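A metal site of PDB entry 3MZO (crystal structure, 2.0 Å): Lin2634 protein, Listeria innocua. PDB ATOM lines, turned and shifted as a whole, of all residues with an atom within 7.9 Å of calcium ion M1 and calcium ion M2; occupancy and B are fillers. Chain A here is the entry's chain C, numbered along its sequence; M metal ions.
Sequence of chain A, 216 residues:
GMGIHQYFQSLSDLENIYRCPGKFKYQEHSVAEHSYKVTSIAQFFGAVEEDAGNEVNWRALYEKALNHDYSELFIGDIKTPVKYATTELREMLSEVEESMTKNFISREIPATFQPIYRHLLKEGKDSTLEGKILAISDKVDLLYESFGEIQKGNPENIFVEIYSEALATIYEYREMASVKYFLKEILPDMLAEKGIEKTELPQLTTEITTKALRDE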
ATOM      1  N   ARG A  19     -12.939  10.726 -23.765  1.00  0.00           N
ATOM      2  CA  ARG A  19     -14.037   9.826 -23.428  1.00  0.00           C
ATOM      3  C   ARG A  19     -13.531   8.737 -22.470  1.00  0.00           C
ATOM      4  O   ARG A  19     -12.348   8.358 -22.516  1.00  0.00           O
ATOM      5  CB  ARG A  19     -14.551   9.157 -24.690  1.00  0.00           C
ATOM      6  CG  ARG A  19     -14.885  10.152 -25.849  1.00  0.00           C
ATOM      7  CD  ARG A  19     -16.310  10.424 -25.912  1.00  0.00           C
ATOM      8  NE  ARG A  19     -17.036   9.184 -26.201  1.00  0.00           N
ATOM      9  CZ  ARG A  19     -18.329   9.016 -26.003  1.00  0.00           C
ATOM     10  NH1 ARG A  19     -19.073  10.020 -25.547  1.00  0.00           N
ATOM     11  NH2 ARG A  19     -18.898   7.851 -26.273  1.00  0.00           N
ATOM     12  N   VAL A  31     -13.435  14.339 -27.164  1.00  0.00           N
ATOM     13  CA  VAL A  31     -14.860  14.681 -27.376  1.00  0.00           C
ATOM     14  C   VAL A  31     -15.012  15.236 -28.789  1.00  0.00           C
ATOM     15  O   VAL A  31     -15.959  14.904 -29.477  1.00  0.00           O
ATOM     16  CB  VAL A  31     -15.366  15.636 -26.317  1.00  0.00           C
ATOM     17  CG1 VAL A  31     -16.767  16.190 -26.664  1.00  0.00           C
ATOM     18  CG2 VAL A  31     -15.356  14.929 -24.962  1.00  0.00           C
ATOM     19  N   HIS A  34     -15.108  12.229 -31.044  1.00  0.00           N
ATOM     20  CA  HIS A  34     -16.397  11.569 -30.819  1.00  0.00           C
ATOM     21  C   HIS A  34     -17.502  12.298 -31.589  1.00  0.00           C
ATOM     22  O   HIS A  34     -18.329  11.652 -32.239  1.00  0.00           O
ATOM     23  CB  HIS A  34     -16.696  11.480 -29.295  1.00  0.00           C
ATOM     24  CG  HIS A  34     -18.121  11.180 -28.969  1.00  0.00           C
ATOM     25  ND1 HIS A  34     -18.699   9.938 -29.171  1.00  0.00           N
ATOM     26  CD2 HIS A  34     -19.114  11.977 -28.506  1.00  0.00           C
ATOM     27  CE1 HIS A  34     -19.971   9.981 -28.808  1.00  0.00           C
ATOM     28  NE2 HIS A  34     -20.252  11.209 -28.400  1.00  0.00           N
ATOM     29  N   SER A  35     -17.491  13.632 -31.532  1.00  0.00           N
ATOM     30  CA  SER A  35     -18.465  14.455 -32.188  1.00  0.00           C
ATOM     31  C   SER A  35     -18.393  14.294 -33.694  1.00  0.00           C
ATOM     32  O   SER A  35     -19.425  14.188 -34.355  1.00  0.00           O
ATOM     33  CB  SER A  35     -18.306  15.918 -31.793  1.00  0.00           C
ATOM     34  OG  SER A  35     -18.497  16.084 -30.386  1.00  0.00           O
ATOM     35  N   VAL A  38     -19.887  10.647 -34.430  1.00  0.00           N
ATOM     36  CA  VAL A  38     -21.352  10.682 -34.232  1.00  0.00           C
ATOM     37  C   VAL A  38     -22.045  11.430 -35.401  1.00  0.00           C
ATOM     38  O   VAL A  38     -23.089  10.993 -35.903  1.00  0.00           O
ATOM     39  CB  VAL A  38     -21.749  11.324 -32.885  1.00  0.00           C
ATOM     40  CG1 VAL A  38     -23.268  11.523 -32.807  1.00  0.00           C
ATOM     41  CG2 VAL A  38     -21.287  10.448 -31.713  1.00  0.00           C
ATOM     42  N   ALA A  65     -26.311  16.382 -33.998  1.00  0.00           N
ATOM     43  CA  ALA A  65     -25.172  15.468 -33.837  1.00  0.00           C
ATOM     44  C   ALA A  65     -23.878  16.248 -33.604  1.00  0.00           C
ATOM     45  O   ALA A  65     -23.122  15.929 -32.681  1.00  0.00           O
ATOM     46  CB  ALA A  65     -25.043  14.526 -35.062  1.00  0.00           C
ATOM     47  N   ASN A  67     -23.263  19.282 -32.380  1.00  0.00           N
ATOM     48  CA  ASN A  67     -23.181  20.094 -31.197  1.00  0.00           C
ATOM     49  C   ASN A  67     -23.523  19.407 -29.868  1.00  0.00           C
ATOM     50  O   ASN A  67     -23.399  20.019 -28.820  1.00  0.00           O
ATOM     51  CB  ASN A  67     -24.082  21.297 -31.393  1.00  0.00           C
ATOM     52  CG  ASN A  67     -23.735  22.055 -32.616  1.00  0.00           C
ATOM     53  OD1 ASN A  67     -22.694  22.719 -32.698  1.00  0.00           O
ATOM     54  ND2 ASN A  67     -24.603  21.978 -33.623  1.00  0.00           N
ATOM     55  N   HIS A  68     -23.902  18.138 -29.919  1.00  0.00           N
ATOM     56  CA  HIS A  68     -24.497  17.473 -28.744  1.00  0.00           C
ATOM     57  C   HIS A  68     -23.579  17.369 -27.548  1.00  0.00           C
ATOM     58  O   HIS A  68     -24.046  17.369 -26.401  1.00  0.00           O
ATOM     59  CB  HIS A  68     -25.064  16.067 -29.065  1.00  0.00           C
ATOM     60  CG  HIS A  68     -24.036  14.985 -29.072  1.00  0.00           C
ATOM     61  ND1 HIS A  68     -23.148  14.807 -30.106  1.00  0.00           N
ATOM     62  CD2 HIS A  68     -23.777  13.998 -28.182  1.00  0.00           C
ATOM     63  CE1 HIS A  68     -22.364  13.779 -29.840  1.00  0.00           C
ATOM     64  NE2 HIS A  68     -22.731  13.261 -28.680  1.00  0.00           N
ATOM     65  N   ASP A  69     -22.282  17.263 -27.782  1.00  0.00           N
ATOM     66  CA  ASP A  69     -21.360  17.168 -26.635  1.00  0.00           C
ATOM     67  C   ASP A  69     -20.460  18.385 -26.411  1.00  0.00           C
ATOM     68  O   ASP A  69     -19.533  18.327 -25.591  1.00  0.00           O
ATOM     69  CB  ASP A  69     -20.567  15.870 -26.717  1.00  0.00           C
ATOM     70  CG  ASP A  69     -21.254  14.724 -25.974  1.00  0.00           C
ATOM     71  OD1 ASP A  69     -22.231  14.941 -25.204  1.00  0.00           O
ATOM     72  OD2 ASP A  69     -20.776  13.590 -26.138  1.00  0.00           O
ATOM     73  N   TYR A  70     -20.782  19.497 -27.064  1.00  0.00           N
ATOM     74  CA  TYR A  70     -20.044  20.725 -26.844  1.00  0.00           C
ATOM     75  C   TYR A  70     -19.999  21.082 -25.368  1.00  0.00           C
ATOM     76  O   TYR A  70     -18.975  21.575 -24.880  1.00  0.00           O
ATOM     77  CB  TYR A  70     -20.654  21.887 -27.639  1.00  0.00           C
ATOM     78  CG  TYR A  70     -19.903  23.190 -27.410  1.00  0.00           C
ATOM     79  CD1 TYR A  70     -18.763  23.499 -28.142  1.00  0.00           C
ATOM     80  CD2 TYR A  70     -20.300  24.066 -26.452  1.00  0.00           C
ATOM     81  CE1 TYR A  70     -18.066  24.678 -27.926  1.00  0.00           C
ATOM     82  CE2 TYR A  70     -19.631  25.257 -26.227  1.00  0.00           C
ATOM     83  CZ  TYR A  70     -18.532  25.567 -26.965  1.00  0.00           C
ATOM     84  OH  TYR A  70     -17.875  26.765 -26.687  1.00  0.00           O
ATOM     85  N   SER A  71     -21.112  20.859 -24.665  1.00  0.00           N
ATOM     86  CA  SER A  71     -21.235  21.219 -23.252  1.00  0.00           C
ATOM     87  C   SER A  71     -20.344  20.402 -22.291  1.00  0.00           C
ATOM     88  O   SER A  71     -20.259  20.713 -21.115  1.00  0.00           O
ATOM     89  CB  SER A  71     -22.697  21.113 -22.784  1.00  0.00           C
ATOM     90  OG  SER A  71     -23.142  19.784 -22.944  1.00  0.00           O
ATOM     91  N   GLU A  72     -19.651  19.375 -22.793  1.00  0.00           N
ATOM     92  CA  GLU A  72     -18.633  18.688 -22.002  1.00  0.00           C
ATOM     93  C   GLU A  72     -17.486  19.634 -21.594  1.00  0.00           C
ATOM     94  O   GLU A  72     -16.742  19.365 -20.654  1.00  0.00           O
ATOM     95  CB  GLU A  72     -18.074  17.499 -22.792  1.00  0.00           C
ATOM     96  CG  GLU A  72     -19.108  16.420 -23.115  1.00  0.00           C
ATOM     97  CD  GLU A  72     -19.759  15.816 -21.864  1.00  0.00           C
ATOM     98  OE1 GLU A  72     -19.011  15.333 -20.982  1.00  0.00           O
ATOM     99  OE2 GLU A  72     -21.016  15.806 -21.780  1.00  0.00           O
ATOM    100  N   ILE A  75     -18.967  20.490 -17.820  1.00  0.00           N
ATOM    101  CA  ILE A  75     -19.018  19.442 -16.780  1.00  0.00           C
ATOM    102  C   ILE A  75     -19.034  18.053 -17.407  1.00  0.00           C
ATOM    103  O   ILE A  75     -19.930  17.760 -18.213  1.00  0.00           O
ATOM    104  CB  ILE A  75     -20.257  19.597 -15.844  1.00  0.00           C
ATOM    105  N   GLU A  97     -24.709  21.842 -15.835  1.00  0.00           N
ATOM    106  CA  GLU A  97     -24.316  21.863 -17.254  1.00  0.00           C
ATOM    107  C   GLU A  97     -25.150  22.922 -17.974  1.00  0.00           C
ATOM    108  O   GLU A  97     -24.606  23.842 -18.588  1.00  0.00           O
ATOM    109  CB  GLU A  97     -24.577  20.479 -17.875  1.00  0.00           C
ATOM    110  CG  GLU A  97     -24.500  20.396 -19.420  1.00  0.00           C
ATOM    111  CD  GLU A  97     -25.649  19.553 -20.046  1.00  0.00           C
ATOM    112  OE1 GLU A  97     -26.630  19.239 -19.316  1.00  0.00           O
ATOM    113  OE2 GLU A  97     -25.584  19.226 -21.269  1.00  0.00           O
ATOM    114  N   LEU A 121     -26.924  24.506 -28.640  1.00  0.00           N
ATOM    115  CA  LEU A 121     -26.293  23.854 -27.489  1.00  0.00           C
ATOM    116  C   LEU A 121     -27.261  23.201 -26.510  1.00  0.00           C
ATOM    117  O   LEU A 121     -26.829  22.548 -25.587  1.00  0.00           O
ATOM    118  CB  LEU A 121     -25.306  24.822 -26.767  1.00  0.00           C
ATOM    119  CG  LEU A 121     -24.254  25.447 -27.687  1.00  0.00           C
ATOM    120  CD1 LEU A 121     -23.369  26.405 -26.893  1.00  0.00           C
ATOM    121  CD2 LEU A 121     -23.408  24.414 -28.394  1.00  0.00           C
ATOM    122  N   LYS A 122     -28.561  23.302 -26.741  1.00  0.00           N
ATOM    123  CA  LYS A 122     -29.524  22.621 -25.868  1.00  0.00           C
ATOM    124  C   LYS A 122     -29.606  21.128 -26.161  1.00  0.00           C
ATOM    125  O   LYS A 122     -29.100  20.663 -27.169  1.00  0.00           O
ATOM    126  CB  LYS A 122     -30.905  23.211 -26.075  1.00  0.00           C
ATOM    127  CG  LYS A 122     -31.605  22.740 -27.335  1.00  0.00           C
ATOM    128  CD  LYS A 122     -32.923  23.460 -27.447  1.00  0.00           C
ATOM    129  CE  LYS A 122     -33.741  22.927 -28.587  1.00  0.00           C
ATOM    130  NZ  LYS A 122     -35.119  23.471 -28.436  1.00  0.00           N
ATOM    131  N   GLU A 123     -30.318  20.399 -25.288  1.00  0.00           N
ATOM    132  CA  GLU A 123     -30.470  18.945 -25.393  1.00  0.00           C
ATOM    133  C   GLU A 123     -31.148  18.602 -26.688  1.00  0.00           C
ATOM    134  O   GLU A 123     -32.248  19.076 -26.950  1.00  0.00           O
ATOM    135  CB  GLU A 123     -31.279  18.370 -24.217  1.00  0.00           C
ATOM    136  CG  GLU A 123     -31.559  16.853 -24.320  1.00  0.00           C
ATOM    137  CD  GLU A 123     -30.262  16.024 -24.377  1.00  0.00           C
ATOM    138  OE1 GLU A 123     -29.367  16.248 -23.528  1.00  0.00           O
ATOM    139  OE2 GLU A 123     -30.120  15.174 -25.280  1.00  0.00           O
ATOM    140  N   GLY A 124     -30.485  17.808 -27.513  1.00  0.00           N
ATOM    141  CA  GLY A 124     -30.992  17.452 -28.809  1.00  0.00           C
ATOM    142  C   GLY A 124     -31.703  16.129 -28.939  1.00  0.00           C
ATOM    143  O   GLY A 124     -32.298  15.887 -29.994  1.00  0.00           O
ATOM    144  N   LYS A 125     -31.627  15.254 -27.924  1.00  0.00           N
ATOM    145  CA  LYS A 125     -32.256  13.932 -28.026  1.00  0.00           C
ATOM    146  C   LYS A 125     -33.704  14.077 -27.631  1.00  0.00           C
ATOM    147  O   LYS A 125     -34.045  14.002 -26.456  1.00  0.00           O
ATOM    148  CB  LYS A 125     -31.576  12.885 -27.137  1.00  0.00           C
ATOM    149  CG  LYS A 125     -30.170  12.520 -27.599  1.00  0.00           C
ATOM    150  CD  LYS A 125     -29.442  11.598 -26.637  1.00  0.00           C
ATOM    151  CE  LYS A 125     -27.970  11.405 -27.067  1.00  0.00           C
ATOM    152  NZ  LYS A 125     -27.254  10.395 -26.195  1.00  0.00           N
ATOM    153  N   LEU A 134     -29.884  11.047 -33.460  1.00  0.00           N
ATOM    154  CA  LEU A 134     -28.777  11.418 -32.578  1.00  0.00           C
ATOM    155  C   LEU A 134     -28.644  10.380 -31.473  1.00  0.00           C
ATOM    156  O   LEU A 134     -27.550   9.972 -31.157  1.00  0.00           O
ATOM    157  CB  LEU A 134     -28.967  12.806 -31.957  1.00  0.00           C
ATOM    158  CG  LEU A 134     -28.086  13.188 -30.761  1.00  0.00           C
ATOM    159  CD1 LEU A 134     -26.606  13.141 -31.165  1.00  0.00           C
ATOM    160  CD2 LEU A 134     -28.534  14.576 -30.241  1.00  0.00           C
ATOM    161  N   SER A 137     -27.051   7.220 -32.945  1.00  0.00           N
ATOM    162  CA  SER A 137     -25.705   7.519 -33.436  1.00  0.00           C
ATOM    163  C   SER A 137     -24.669   7.634 -32.294  1.00  0.00           C
ATOM    164  O   SER A 137     -23.548   7.148 -32.406  1.00  0.00           O
ATOM    165  CB  SER A 137     -25.745   8.794 -34.282  1.00  0.00           C
ATOM    166  OG  SER A 137     -26.515   8.586 -35.455  1.00  0.00           O
ATOM    167  N   ASP A 138     -25.060   8.313 -31.219  1.00  0.00           N
ATOM    168  CA  ASP A 138     -24.267   8.408 -30.024  1.00  0.00           C
ATOM    169  C   ASP A 138     -23.966   7.025 -29.461  1.00  0.00           C
ATOM    170  O   ASP A 138     -22.832   6.716 -29.088  1.00  0.00           O
ATOM    171  CB  ASP A 138     -25.009   9.269 -29.000  1.00  0.00           C
ATOM    172  CG  ASP A 138     -24.112   9.698 -27.817  1.00  0.00           C
ATOM    173  OD1 ASP A 138     -22.894   9.695 -27.986  1.00  0.00           O
ATOM    174  OD2 ASP A 138     -24.597  10.059 -26.722  1.00  0.00           O
ATOM    175  N   LYS A 139     -24.981   6.164 -29.393  1.00  0.00           N
ATOM    176  CA  LYS A 139     -24.809   4.815 -28.901  1.00  0.00           C
ATOM    177  C   LYS A 139     -24.047   3.935 -29.855  1.00  0.00           C
ATOM    178  O   LYS A 139     -23.317   3.049 -29.398  1.00  0.00           O
ATOM    179  CB  LYS A 139     -26.137   4.170 -28.523  1.00  0.00           C
ATOM    180  CG  LYS A 139     -26.770   4.842 -27.345  1.00  0.00           C
ATOM    181  CD  LYS A 139     -25.898   4.834 -26.106  1.00  0.00           C
ATOM    182  CE  LYS A 139     -26.580   5.552 -24.963  1.00  0.00           C
ATOM    183  NZ  LYS A 139     -25.693   5.591 -23.791  1.00  0.00           N
ATOM    184  N   ASP A 141     -21.577   4.996 -31.728  1.00  0.00           N
ATOM    185  CA  ASP A 141     -20.187   5.324 -31.457  1.00  0.00           C
ATOM    186  C   ASP A 141     -19.681   4.639 -30.187  1.00  0.00           C
ATOM    187  O   ASP A 141     -18.602   4.076 -30.188  1.00  0.00           O
ATOM    188  CB  ASP A 141     -19.942   6.817 -31.342  1.00  0.00           C
ATOM    189  CG  ASP A 141     -18.420   7.131 -31.339  1.00  0.00           C
ATOM    190  OD1 ASP A 141     -17.699   6.511 -32.181  1.00  0.00           O
ATOM    191  OD2 ASP A 141     -17.966   7.953 -30.486  1.00  0.00           O
ATOM    192  N   LEU A 142     -20.464   4.687 -29.116  1.00  0.00           N
ATOM    193  CA  LEU A 142     -20.115   4.048 -27.853  1.00  0.00           C
ATOM    194  C   LEU A 142     -19.904   2.569 -28.039  1.00  0.00           C
ATOM    195  O   LEU A 142     -18.990   1.989 -27.452  1.00  0.00           O
ATOM    196  CB  LEU A 142     -21.221   4.311 -26.806  1.00  0.00           C
ATOM    197  CG  LEU A 142     -20.959   3.958 -25.347  1.00  0.00           C
ATOM    198  CD1 LEU A 142     -19.702   4.676 -24.805  1.00  0.00           C
ATOM    199  CD2 LEU A 142     -22.202   4.282 -24.497  1.00  0.00           C
ATOM    200  N   GLU A 145     -16.537   2.100 -29.762  1.00  0.00           N
ATOM    201  CA  GLU A 145     -15.396   2.392 -28.890  1.00  0.00           C
ATOM    202  C   GLU A 145     -15.141   1.185 -27.977  1.00  0.00           C
ATOM    203  O   GLU A 145     -14.001   0.752 -27.799  1.00  0.00           O
ATOM    204  CB  GLU A 145     -15.673   3.561 -27.958  1.00  0.00           C
ATOM    205  CG  GLU A 145     -15.815   4.930 -28.558  1.00  0.00           C
ATOM    206  CD  GLU A 145     -16.183   5.969 -27.477  1.00  0.00           C
ATOM    207  OE1 GLU A 145     -17.132   5.748 -26.719  1.00  0.00           O
ATOM    208  OE2 GLU A 145     -15.530   7.016 -27.381  1.00  0.00           O
HETATM  209 CA    CA M   1     -22.146  11.652 -26.530  1.00  0.00          CA
HETATM  210 CA    CA M   2     -24.041  16.149 -24.189  1.00  0.00          CA
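Calcium ion M1 is bound by OD2 of Asp 69 (2.4 Å), OD1 of Asp 138 (2.6 Å), NE2 of His 34 (2.7 Å) and NE2 of His 68 (2.7 Å). Slightly farther from calcium ion M1 lies OD2 of Asp 138 (2.9 Å).
Residues that only touch calcium ion M2: Glu 72 and Ser 71. Four residues have an atom within 4 Å of calcium ion M2: His 68, Asp 69, Ser 71 and Glu 72. The nearest printed residue that does not touch calcium ion M2 is Glu 97 (4.5 Å).
The side-chain carboxylate (OD1) of Asp 69 is bound to calcium ion M2, at 2.4 Å. O of His 68 is bound to calcium ion M2 (2.5 Å). Calcium ion M2 has two donor atoms within binding distance.
Merely in contact with calcium ion M1: Arg 19 (3.6 Å). Within 4 Å of calcium ion M1: Arg 19, His 34, His 68, Asp 69 and Asp 138.
NH2 of Arg 19 lies within salt-bridge range of OE1 of Glu 145 (2.8 Å). The guanidinium group (NH1) of Arg 19 sits close to the side-chain carboxylate (OD2) of Asp 69 (3.999 Å). OE2 of Glu 97 sits at hydrogen-bond distance from OG of Ser 71, 3.0 Å away. O of Ala 65 is in hydrogen-bond range of ND1 of His 68. ND1 of His 34 is in hydrogen-bond range of OD2 of Asp 141 (2.5 Å). A ring nitrogen (ND1) of His 34 sits close to the guanidinium group (NE) of Arg 19 (3.5 Å). OD2 of Asp 138 lies within salt-bridge range of NZ of Lys 125, 2.7 Å away.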
